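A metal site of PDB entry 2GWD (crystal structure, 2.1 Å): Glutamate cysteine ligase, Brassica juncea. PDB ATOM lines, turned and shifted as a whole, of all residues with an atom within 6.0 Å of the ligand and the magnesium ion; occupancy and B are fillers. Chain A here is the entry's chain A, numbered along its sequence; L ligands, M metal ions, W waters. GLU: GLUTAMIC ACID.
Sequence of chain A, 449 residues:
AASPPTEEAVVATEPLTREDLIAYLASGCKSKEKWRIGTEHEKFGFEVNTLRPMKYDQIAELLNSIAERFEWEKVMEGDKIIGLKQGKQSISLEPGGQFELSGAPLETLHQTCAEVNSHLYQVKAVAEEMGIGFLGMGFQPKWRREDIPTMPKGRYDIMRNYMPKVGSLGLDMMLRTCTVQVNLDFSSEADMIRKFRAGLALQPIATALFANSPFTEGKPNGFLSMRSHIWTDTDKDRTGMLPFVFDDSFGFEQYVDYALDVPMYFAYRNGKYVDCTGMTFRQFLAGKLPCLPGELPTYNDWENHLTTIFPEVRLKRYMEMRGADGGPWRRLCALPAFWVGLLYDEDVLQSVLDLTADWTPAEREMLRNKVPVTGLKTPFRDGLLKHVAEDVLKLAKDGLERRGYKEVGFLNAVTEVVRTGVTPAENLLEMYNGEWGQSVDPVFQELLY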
ATOM      1  N   GLU A  40     -25.376  23.110  26.654  1.00  0.00           N
ATOM      2  CA  GLU A  40     -24.738  22.142  27.541  1.00  0.00           C
ATOM      3  C   GLU A  40     -23.267  22.040  27.196  1.00  0.00           C
ATOM      4  O   GLU A  40     -22.897  22.015  26.011  1.00  0.00           O
ATOM      5  CB  GLU A  40     -25.300  20.741  27.397  1.00  0.00           C
ATOM      6  CG  GLU A  40     -26.786  20.584  27.467  1.00  0.00           C
ATOM      7  CD  GLU A  40     -27.220  19.111  27.385  1.00  0.00           C
ATOM      8  OE1 GLU A  40     -26.368  18.204  27.259  1.00  0.00           O
ATOM      9  OE2 GLU A  40     -28.451  18.879  27.390  1.00  0.00           O
ATOM     10  N   GLU A  42     -19.380  20.116  28.819  1.00  0.00           N
ATOM     11  CA  GLU A  42     -18.739  19.161  29.700  1.00  0.00           C
ATOM     12  C   GLU A  42     -17.260  19.554  29.817  1.00  0.00           C
ATOM     13  O   GLU A  42     -16.669  20.045  28.837  1.00  0.00           O
ATOM     14  CB  GLU A  42     -18.845  17.738  29.103  1.00  0.00           C
ATOM     15  CG  GLU A  42     -20.262  17.242  28.964  1.00  0.00           C
ATOM     16  CD  GLU A  42     -20.433  16.123  27.958  1.00  0.00           C
ATOM     17  OE1 GLU A  42     -19.505  15.869  27.178  1.00  0.00           O
ATOM     18  OE2 GLU A  42     -21.533  15.490  27.962  1.00  0.00           O
ATOM     19  N   SER A  92     -24.420  17.989  36.210  1.00  0.00           N
ATOM     20  CA  SER A  92     -24.439  16.533  36.193  1.00  0.00           C
ATOM     21  C   SER A  92     -23.056  15.964  35.849  1.00  0.00           C
ATOM     22  O   SER A  92     -22.100  16.713  35.618  1.00  0.00           O
ATOM     23  CB  SER A  92     -25.500  16.054  35.202  1.00  0.00           C
ATOM     24  OG  SER A  92     -25.070  16.246  33.880  1.00  0.00           O
ATOM     25  N   GLU A  94     -20.886  13.081  33.595  1.00  0.00           N
ATOM     26  CA  GLU A  94     -20.709  12.048  32.589  1.00  0.00           C
ATOM     27  C   GLU A  94     -19.901  10.877  33.208  1.00  0.00           C
ATOM     28  O   GLU A  94     -19.386  11.008  34.312  1.00  0.00           O
ATOM     29  CB  GLU A  94     -20.076  12.639  31.347  1.00  0.00           C
ATOM     30  CG  GLU A  94     -20.974  13.629  30.594  1.00  0.00           C
ATOM     31  CD  GLU A  94     -22.226  12.980  29.994  1.00  0.00           C
ATOM     32  OE1 GLU A  94     -22.250  11.745  29.812  1.00  0.00           O
ATOM     33  OE2 GLU A  94     -23.190  13.705  29.697  1.00  0.00           O
ATOM     34  N   GLN A  98     -16.700  13.700  33.857  1.00  0.00           N
ATOM     35  CA  GLN A  98     -16.761  14.953  33.107  1.00  0.00           C
ATOM     36  C   GLN A  98     -17.898  15.763  33.715  1.00  0.00           C
ATOM     37  O   GLN A  98     -18.979  15.238  34.006  1.00  0.00           O
ATOM     38  CB  GLN A  98     -16.956  14.752  31.602  1.00  0.00           C
ATOM     39  CG  GLN A  98     -15.968  13.773  30.933  1.00  0.00           C
ATOM     40  CD  GLN A  98     -16.543  12.378  30.842  1.00  0.00           C
ATOM     41  OE1 GLN A  98     -16.910  11.783  31.859  1.00  0.00           O
ATOM     42  NE2 GLN A  98     -16.630  11.843  29.597  1.00  0.00           N
ATOM     43  N   GLU A 100     -20.588  18.516  33.932  1.00  0.00           N
ATOM     44  CA  GLU A 100     -21.510  19.128  32.985  1.00  0.00           C
ATOM     45  C   GLU A 100     -22.438  20.176  33.584  1.00  0.00           C
ATOM     46  O   GLU A 100     -23.003  19.963  34.642  1.00  0.00           O
ATOM     47  CB  GLU A 100     -22.409  18.053  32.401  1.00  0.00           C
ATOM     48  CG  GLU A 100     -23.466  18.604  31.450  1.00  0.00           C
ATOM     49  CD  GLU A 100     -24.166  17.515  30.694  1.00  0.00           C
ATOM     50  OE1 GLU A 100     -23.441  16.674  30.127  1.00  0.00           O
ATOM     51  OE2 GLU A 100     -25.415  17.468  30.683  1.00  0.00           O
ATOM     52  N   GLY A 138     -11.852  18.271  23.757  1.00  0.00           N
ATOM     53  CA  GLY A 138     -12.762  17.244  23.292  1.00  0.00           C
ATOM     54  C   GLY A 138     -12.451  15.835  23.736  1.00  0.00           C
ATOM     55  O   GLY A 138     -13.341  14.987  23.763  1.00  0.00           O
ATOM     56  N   MET A 173     -15.793   7.108  24.418  1.00  0.00           N
ATOM     57  CA  MET A 173     -16.845   8.073  24.381  1.00  0.00           C
ATOM     58  C   MET A 173     -17.263   8.380  25.818  1.00  0.00           C
ATOM     59  O   MET A 173     -17.242   9.537  26.248  1.00  0.00           O
ATOM     60  CB  MET A 173     -18.041   7.561  23.567  1.00  0.00           C
ATOM     61  CG  MET A 173     -19.156   8.591  23.410  1.00  0.00           C
ATOM     62  SD  MET A 173     -20.254   8.595  24.858  1.00  0.00           S
ATOM     63  CE  MET A 173     -21.224   7.137  24.510  1.00  0.00           C
ATOM     64  N   MET A 174     -17.575   7.337  26.570  1.00  0.00           N
ATOM     65  CA  MET A 174     -18.126   7.509  27.907  1.00  0.00           C
ATOM     66  C   MET A 174     -17.155   8.169  28.880  1.00  0.00           C
ATOM     67  O   MET A 174     -17.531   9.087  29.608  1.00  0.00           O
ATOM     68  CB  MET A 174     -18.526   6.136  28.460  1.00  0.00           C
ATOM     69  CG  MET A 174     -19.712   5.562  27.772  1.00  0.00           C
ATOM     70  SD  MET A 174     -20.215   4.026  28.540  1.00  0.00           S
ATOM     71  CE  MET A 174     -20.799   4.589  30.143  1.00  0.00           C
ATOM     72  N   THR A 177     -14.342  11.725  26.556  1.00  0.00           N
ATOM     73  CA  THR A 177     -14.741  12.836  25.685  1.00  0.00           C
ATOM     74  C   THR A 177     -15.549  13.909  26.404  1.00  0.00           C
ATOM     75  O   THR A 177     -16.206  13.644  27.419  1.00  0.00           O
ATOM     76  CB  THR A 177     -15.542  12.379  24.421  1.00  0.00           C
ATOM     77  OG1 THR A 177     -16.833  11.874  24.774  1.00  0.00           O
ATOM     78  CG2 THR A 177     -14.782  11.352  23.636  1.00  0.00           C
ATOM     79  N   CYS A 178     -15.487  15.121  25.886  1.00  0.00           N
ATOM     80  CA  CYS A 178     -16.292  16.256  26.342  1.00  0.00           C
ATOM     81  C   CYS A 178     -16.856  17.001  25.141  1.00  0.00           C
ATOM     82  O   CYS A 178     -16.113  17.284  24.211  1.00  0.00           O
ATOM     83  CB  CYS A 178     -15.434  17.252  27.118  1.00  0.00           C
ATOM     84  SG  CYS A 178     -15.197  16.924  28.851  1.00  0.00           S
ATOM     85  N   THR A 179     -18.140  17.346  25.200  1.00  0.00           N
ATOM     86  CA  THR A 179     -18.815  18.104  24.154  1.00  0.00           C
ATOM     87  C   THR A 179     -19.267  19.479  24.656  1.00  0.00           C
ATOM     88  O   THR A 179     -19.376  19.726  25.866  1.00  0.00           O
ATOM     89  CB  THR A 179     -20.095  17.367  23.608  1.00  0.00           C
ATOM     90  OG1 THR A 179     -20.596  18.034  22.436  1.00  0.00           O
ATOM     91  CG2 THR A 179     -21.195  17.366  24.609  1.00  0.00           C
ATOM     92  N   GLN A 181     -22.733  21.410  23.358  1.00  0.00           N
ATOM     93  CA  GLN A 181     -23.891  21.337  22.477  1.00  0.00           C
ATOM     94  C   GLN A 181     -24.919  22.422  22.753  1.00  0.00           C
ATOM     95  O   GLN A 181     -24.875  23.152  23.760  1.00  0.00           O
ATOM     96  CB  GLN A 181     -24.556  19.961  22.548  1.00  0.00           C
ATOM     97  CG  GLN A 181     -25.258  19.638  23.826  1.00  0.00           C
ATOM     98  CD  GLN A 181     -25.853  18.243  23.772  1.00  0.00           C
ATOM     99  OE1 GLN A 181     -25.136  17.235  23.868  1.00  0.00           O
ATOM    100  NE2 GLN A 181     -27.173  18.166  23.611  1.00  0.00           N
ATOM    101  N   ARG A 227     -12.417  12.884  19.353  1.00  0.00           N
ATOM    102  CA  ARG A 227     -13.757  12.789  19.918  1.00  0.00           C
ATOM    103  C   ARG A 227     -14.779  12.419  18.841  1.00  0.00           C
ATOM    104  O   ARG A 227     -15.527  11.459  19.018  1.00  0.00           O
ATOM    105  CB  ARG A 227     -14.161  14.093  20.598  1.00  0.00           C
ATOM    106  CG  ARG A 227     -15.592  14.112  21.061  1.00  0.00           C
ATOM    107  CD  ARG A 227     -16.051  15.471  21.578  1.00  0.00           C
ATOM    108  NE  ARG A 227     -17.499  15.522  21.513  1.00  0.00           N
ATOM    109  CZ  ARG A 227     -18.192  15.853  20.424  1.00  0.00           C
ATOM    110  NH1 ARG A 227     -17.570  16.284  19.327  1.00  0.00           N
ATOM    111  NH2 ARG A 227     -19.501  15.785  20.432  1.00  0.00           N
ATOM    112  N   TRP A 231     -17.049   8.653  18.025  1.00  0.00           N
ATOM    113  CA  TRP A 231     -18.466   8.460  17.757  1.00  0.00           C
ATOM    114  C   TRP A 231     -18.775   7.651  16.507  1.00  0.00           C
ATOM    115  O   TRP A 231     -19.948   7.362  16.243  1.00  0.00           O
ATOM    116  CB  TRP A 231     -19.167   9.812  17.700  1.00  0.00           C
ATOM    117  CG  TRP A 231     -19.481  10.395  19.033  1.00  0.00           C
ATOM    118  CD1 TRP A 231     -18.890  11.480  19.603  1.00  0.00           C
ATOM    119  CD2 TRP A 231     -20.493   9.956  19.933  1.00  0.00           C
ATOM    120  NE1 TRP A 231     -19.468  11.745  20.817  1.00  0.00           N
ATOM    121  CE2 TRP A 231     -20.455  10.819  21.052  1.00  0.00           C
ATOM    122  CE3 TRP A 231     -21.424   8.916  19.914  1.00  0.00           C
ATOM    123  CZ2 TRP A 231     -21.318  10.675  22.138  1.00  0.00           C
ATOM    124  CZ3 TRP A 231     -22.273   8.767  20.980  1.00  0.00           C
ATOM    125  CH2 TRP A 231     -22.229   9.645  22.084  1.00  0.00           C
ATOM    126  N   THR A 307     -33.023   9.552  24.988  1.00  0.00           N
ATOM    127  CA  THR A 307     -31.790  10.174  25.477  1.00  0.00           C
ATOM    128  C   THR A 307     -30.635   9.140  25.438  1.00  0.00           C
ATOM    129  O   THR A 307     -29.478   9.460  25.740  1.00  0.00           O
ATOM    130  CB  THR A 307     -32.039  10.777  26.899  1.00  0.00           C
ATOM    131  OG1 THR A 307     -33.165  11.677  26.821  1.00  0.00           O
ATOM    132  CG2 THR A 307     -30.859  11.543  27.446  1.00  0.00           C
ATOM    133  N   PHE A 310     -27.784   8.672  20.026  1.00  0.00           N
ATOM    134  CA  PHE A 310     -26.693   9.610  19.923  1.00  0.00           C
ATOM    135  C   PHE A 310     -26.270   9.947  18.479  1.00  0.00           C
ATOM    136  O   PHE A 310     -25.112   9.814  18.150  1.00  0.00           O
ATOM    137  CB  PHE A 310     -25.481   9.074  20.686  1.00  0.00           C
ATOM    138  CG  PHE A 310     -25.748   8.653  22.121  1.00  0.00           C
ATOM    139  CD1 PHE A 310     -26.180   9.578  23.072  1.00  0.00           C
ATOM    140  CD2 PHE A 310     -25.463   7.351  22.533  1.00  0.00           C
ATOM    141  CE1 PHE A 310     -26.370   9.205  24.403  1.00  0.00           C
ATOM    142  CE2 PHE A 310     -25.665   6.960  23.854  1.00  0.00           C
ATOM    143  CZ  PHE A 310     -26.116   7.888  24.801  1.00  0.00           C
ATOM    144  N   ARG A 314     -29.750  15.098  17.289  1.00  0.00           N
ATOM    145  CA  ARG A 314     -30.717  14.290  17.976  1.00  0.00           C
ATOM    146  C   ARG A 314     -32.047  15.030  18.061  1.00  0.00           C
ATOM    147  O   ARG A 314     -32.068  16.228  18.273  1.00  0.00           O
ATOM    148  CB  ARG A 314     -30.209  13.950  19.375  1.00  0.00           C
ATOM    149  CG  ARG A 314     -31.208  13.242  20.255  1.00  0.00           C
ATOM    150  CD  ARG A 314     -30.885  13.510  21.711  1.00  0.00           C
ATOM    151  NE  ARG A 314     -30.070  12.485  22.233  1.00  0.00           N
ATOM    152  CZ  ARG A 314     -29.545  12.475  23.452  1.00  0.00           C
ATOM    153  NH1 ARG A 314     -29.665  13.488  24.306  1.00  0.00           N
ATOM    154  NH2 ARG A 314     -28.872  11.392  23.795  1.00  0.00           N
ATOM    155  N   ARG A 322     -24.902  18.052  18.039  1.00  0.00           N
ATOM    156  CA  ARG A 322     -24.131  17.154  18.900  1.00  0.00           C
ATOM    157  C   ARG A 322     -22.703  16.991  18.395  1.00  0.00           C
ATOM    158  O   ARG A 322     -22.067  15.965  18.636  1.00  0.00           O
ATOM    159  CB  ARG A 322     -24.823  15.783  18.998  1.00  0.00           C
ATOM    160  CG  ARG A 322     -26.110  15.790  19.793  1.00  0.00           C
ATOM    161  CD  ARG A 322     -26.723  14.422  19.991  1.00  0.00           C
ATOM    162  NE  ARG A 322     -25.749  13.450  20.501  1.00  0.00           N
ATOM    163  CZ  ARG A 322     -25.553  13.204  21.790  1.00  0.00           C
ATOM    164  NH1 ARG A 322     -26.253  13.856  22.711  1.00  0.00           N
ATOM    165  NH2 ARG A 322     -24.646  12.313  22.162  1.00  0.00           N
ATOM    166  N   ALA A 324     -19.753  18.906  18.325  1.00  0.00           N
ATOM    167  CA  ALA A 324     -18.659  19.836  18.579  1.00  0.00           C
ATOM    168  C   ALA A 324     -17.858  19.430  19.808  1.00  0.00           C
ATOM    169  O   ALA A 324     -18.415  18.975  20.798  1.00  0.00           O
ATOM    170  CB  ALA A 324     -19.193  21.255  18.732  1.00  0.00           C
HETATM  171  N   GLU L   1     -19.372  13.416  26.277  1.00  0.00           N
HETATM  172  CA  GLU L   1     -19.945  13.152  24.943  1.00  0.00           C
HETATM  173  C   GLU L   1     -19.125  13.857  23.823  1.00  0.00           C
HETATM  174  O   GLU L   1     -19.672  13.971  22.715  1.00  0.00           O
HETATM  175  CB  GLU L   1     -21.427  13.562  24.918  1.00  0.00           C
HETATM  176  CG  GLU L   1     -22.174  12.770  26.024  1.00  0.00           C
HETATM  177  CD  GLU L   1     -23.670  13.093  26.078  1.00  0.00           C
HETATM  178  OE1 GLU L   1     -24.443  12.280  25.500  1.00  0.00           O
HETATM  179  OE2 GLU L   1     -24.002  14.140  26.716  1.00  0.00           O
HETATM  180  OXT GLU L   1     -17.990  14.270  24.069  1.00  0.00           O
HETATM  181 MG    MG M   1     -23.497  15.327  28.514  1.00  0.00          MG
HETATM  182  O   HOH W   1     -23.780  17.182  27.223  1.00  0.00           O
HETATM  183  O   HOH W   2     -27.008  12.183  26.074  1.00  0.00           O
HETATM  184  O   HOH W   3     -25.809  15.290  28.662  1.00  0.00           O
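Water W3 bridges the side-chain carboxylate of Glu 100 (3.0 Å) and the side-chain carboxylate of Glu 40 (3.3 Å). Water W2 bridges an oxygen (OE1) of the ligand and the guanidinium group of Arg 314.
The magnesium ion is bound by OE2 of Glu 94 (2.0 Å). OE2 of Glu 42 binds the magnesium ion (2.0 Å). The magnesium ion is bound by OE1 of Glu 100, at 2.1 Å. OE2 of the ligand binds the magnesium ion, 2.2 Å away. The magnesium ion is bound by water W1 (2.3 Å). Water W3 is bound to the magnesium ion (2.3 Å).
An oxygen (O) of the ligand lies within hydrogen-bond range of the indole nitrogen (NE1) of Trp 231 (2.9 Å). The side-chain hydroxyl of Thr 177 sits at hydrogen-bond distance from an oxygen (OXT) of the ligand (2.8 Å). The guanidinium group of Arg 227 is in salt-bridge range of an oxygen (OXT) of the ligand, at 2.9 Å. N of Thr 179 sits at hydrogen-bond distance from OXT of the ligand (3.3 Å). O of Thr 177 lies within hydrogen-bond range of N of the ligand (3.4 Å). OE1 of the ligand lies within salt-bridge range of NH2 of Arg 322 (3.3 Å). N of Cys 178 lies close to OXT of the ligand.
Residues that only touch the ligand: Phe 310 (3.8 Å). Hydrophobic or aromatic side chains that line the ligand: Trp 231 and Phe 310. Of the 20 residues printed, 9 come within 4 Å of the ligand.
Of the 20 residues printed, 3 come within 4 Å of the magnesium ion.
The side-chain hydroxyl (OG1) of Thr 179 sits at hydrogen-bond distance from the backbone carbonyl oxygen (O) of Ala 324 (2.9 Å). OE1 of Glu 42 lies within hydrogen-bond range of N of Thr 179. N of Cys 178 sits at hydrogen-bond distance from O of Gly 138. The backbone carbonyl oxygen of Glu 42 sits at hydrogen-bond distance from the side-chain sulfur of Cys 178 (3.5 Å). The guanidinium group (NH2) of Arg 227 sits at hydrogen-bond distance from the side-chain hydroxyl (OG1) of Thr 179 (3.2 Å). The side-chain amide nitrogen of Gln 98 is in hydrogen-bond range of the backbone carbonyl oxygen of Thr 177 (2.9 Å). The side-chain hydroxyl (OG1) of Thr 177 lies within hydrogen-bond range of the backbone carbonyl oxygen (O) of Met 173, at 2.8 Å. The guanidinium group (NH2) of Arg 227 lies within hydrogen-bond range of the backbone carbonyl oxygen (O) of Arg 322 (3.1 Å).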
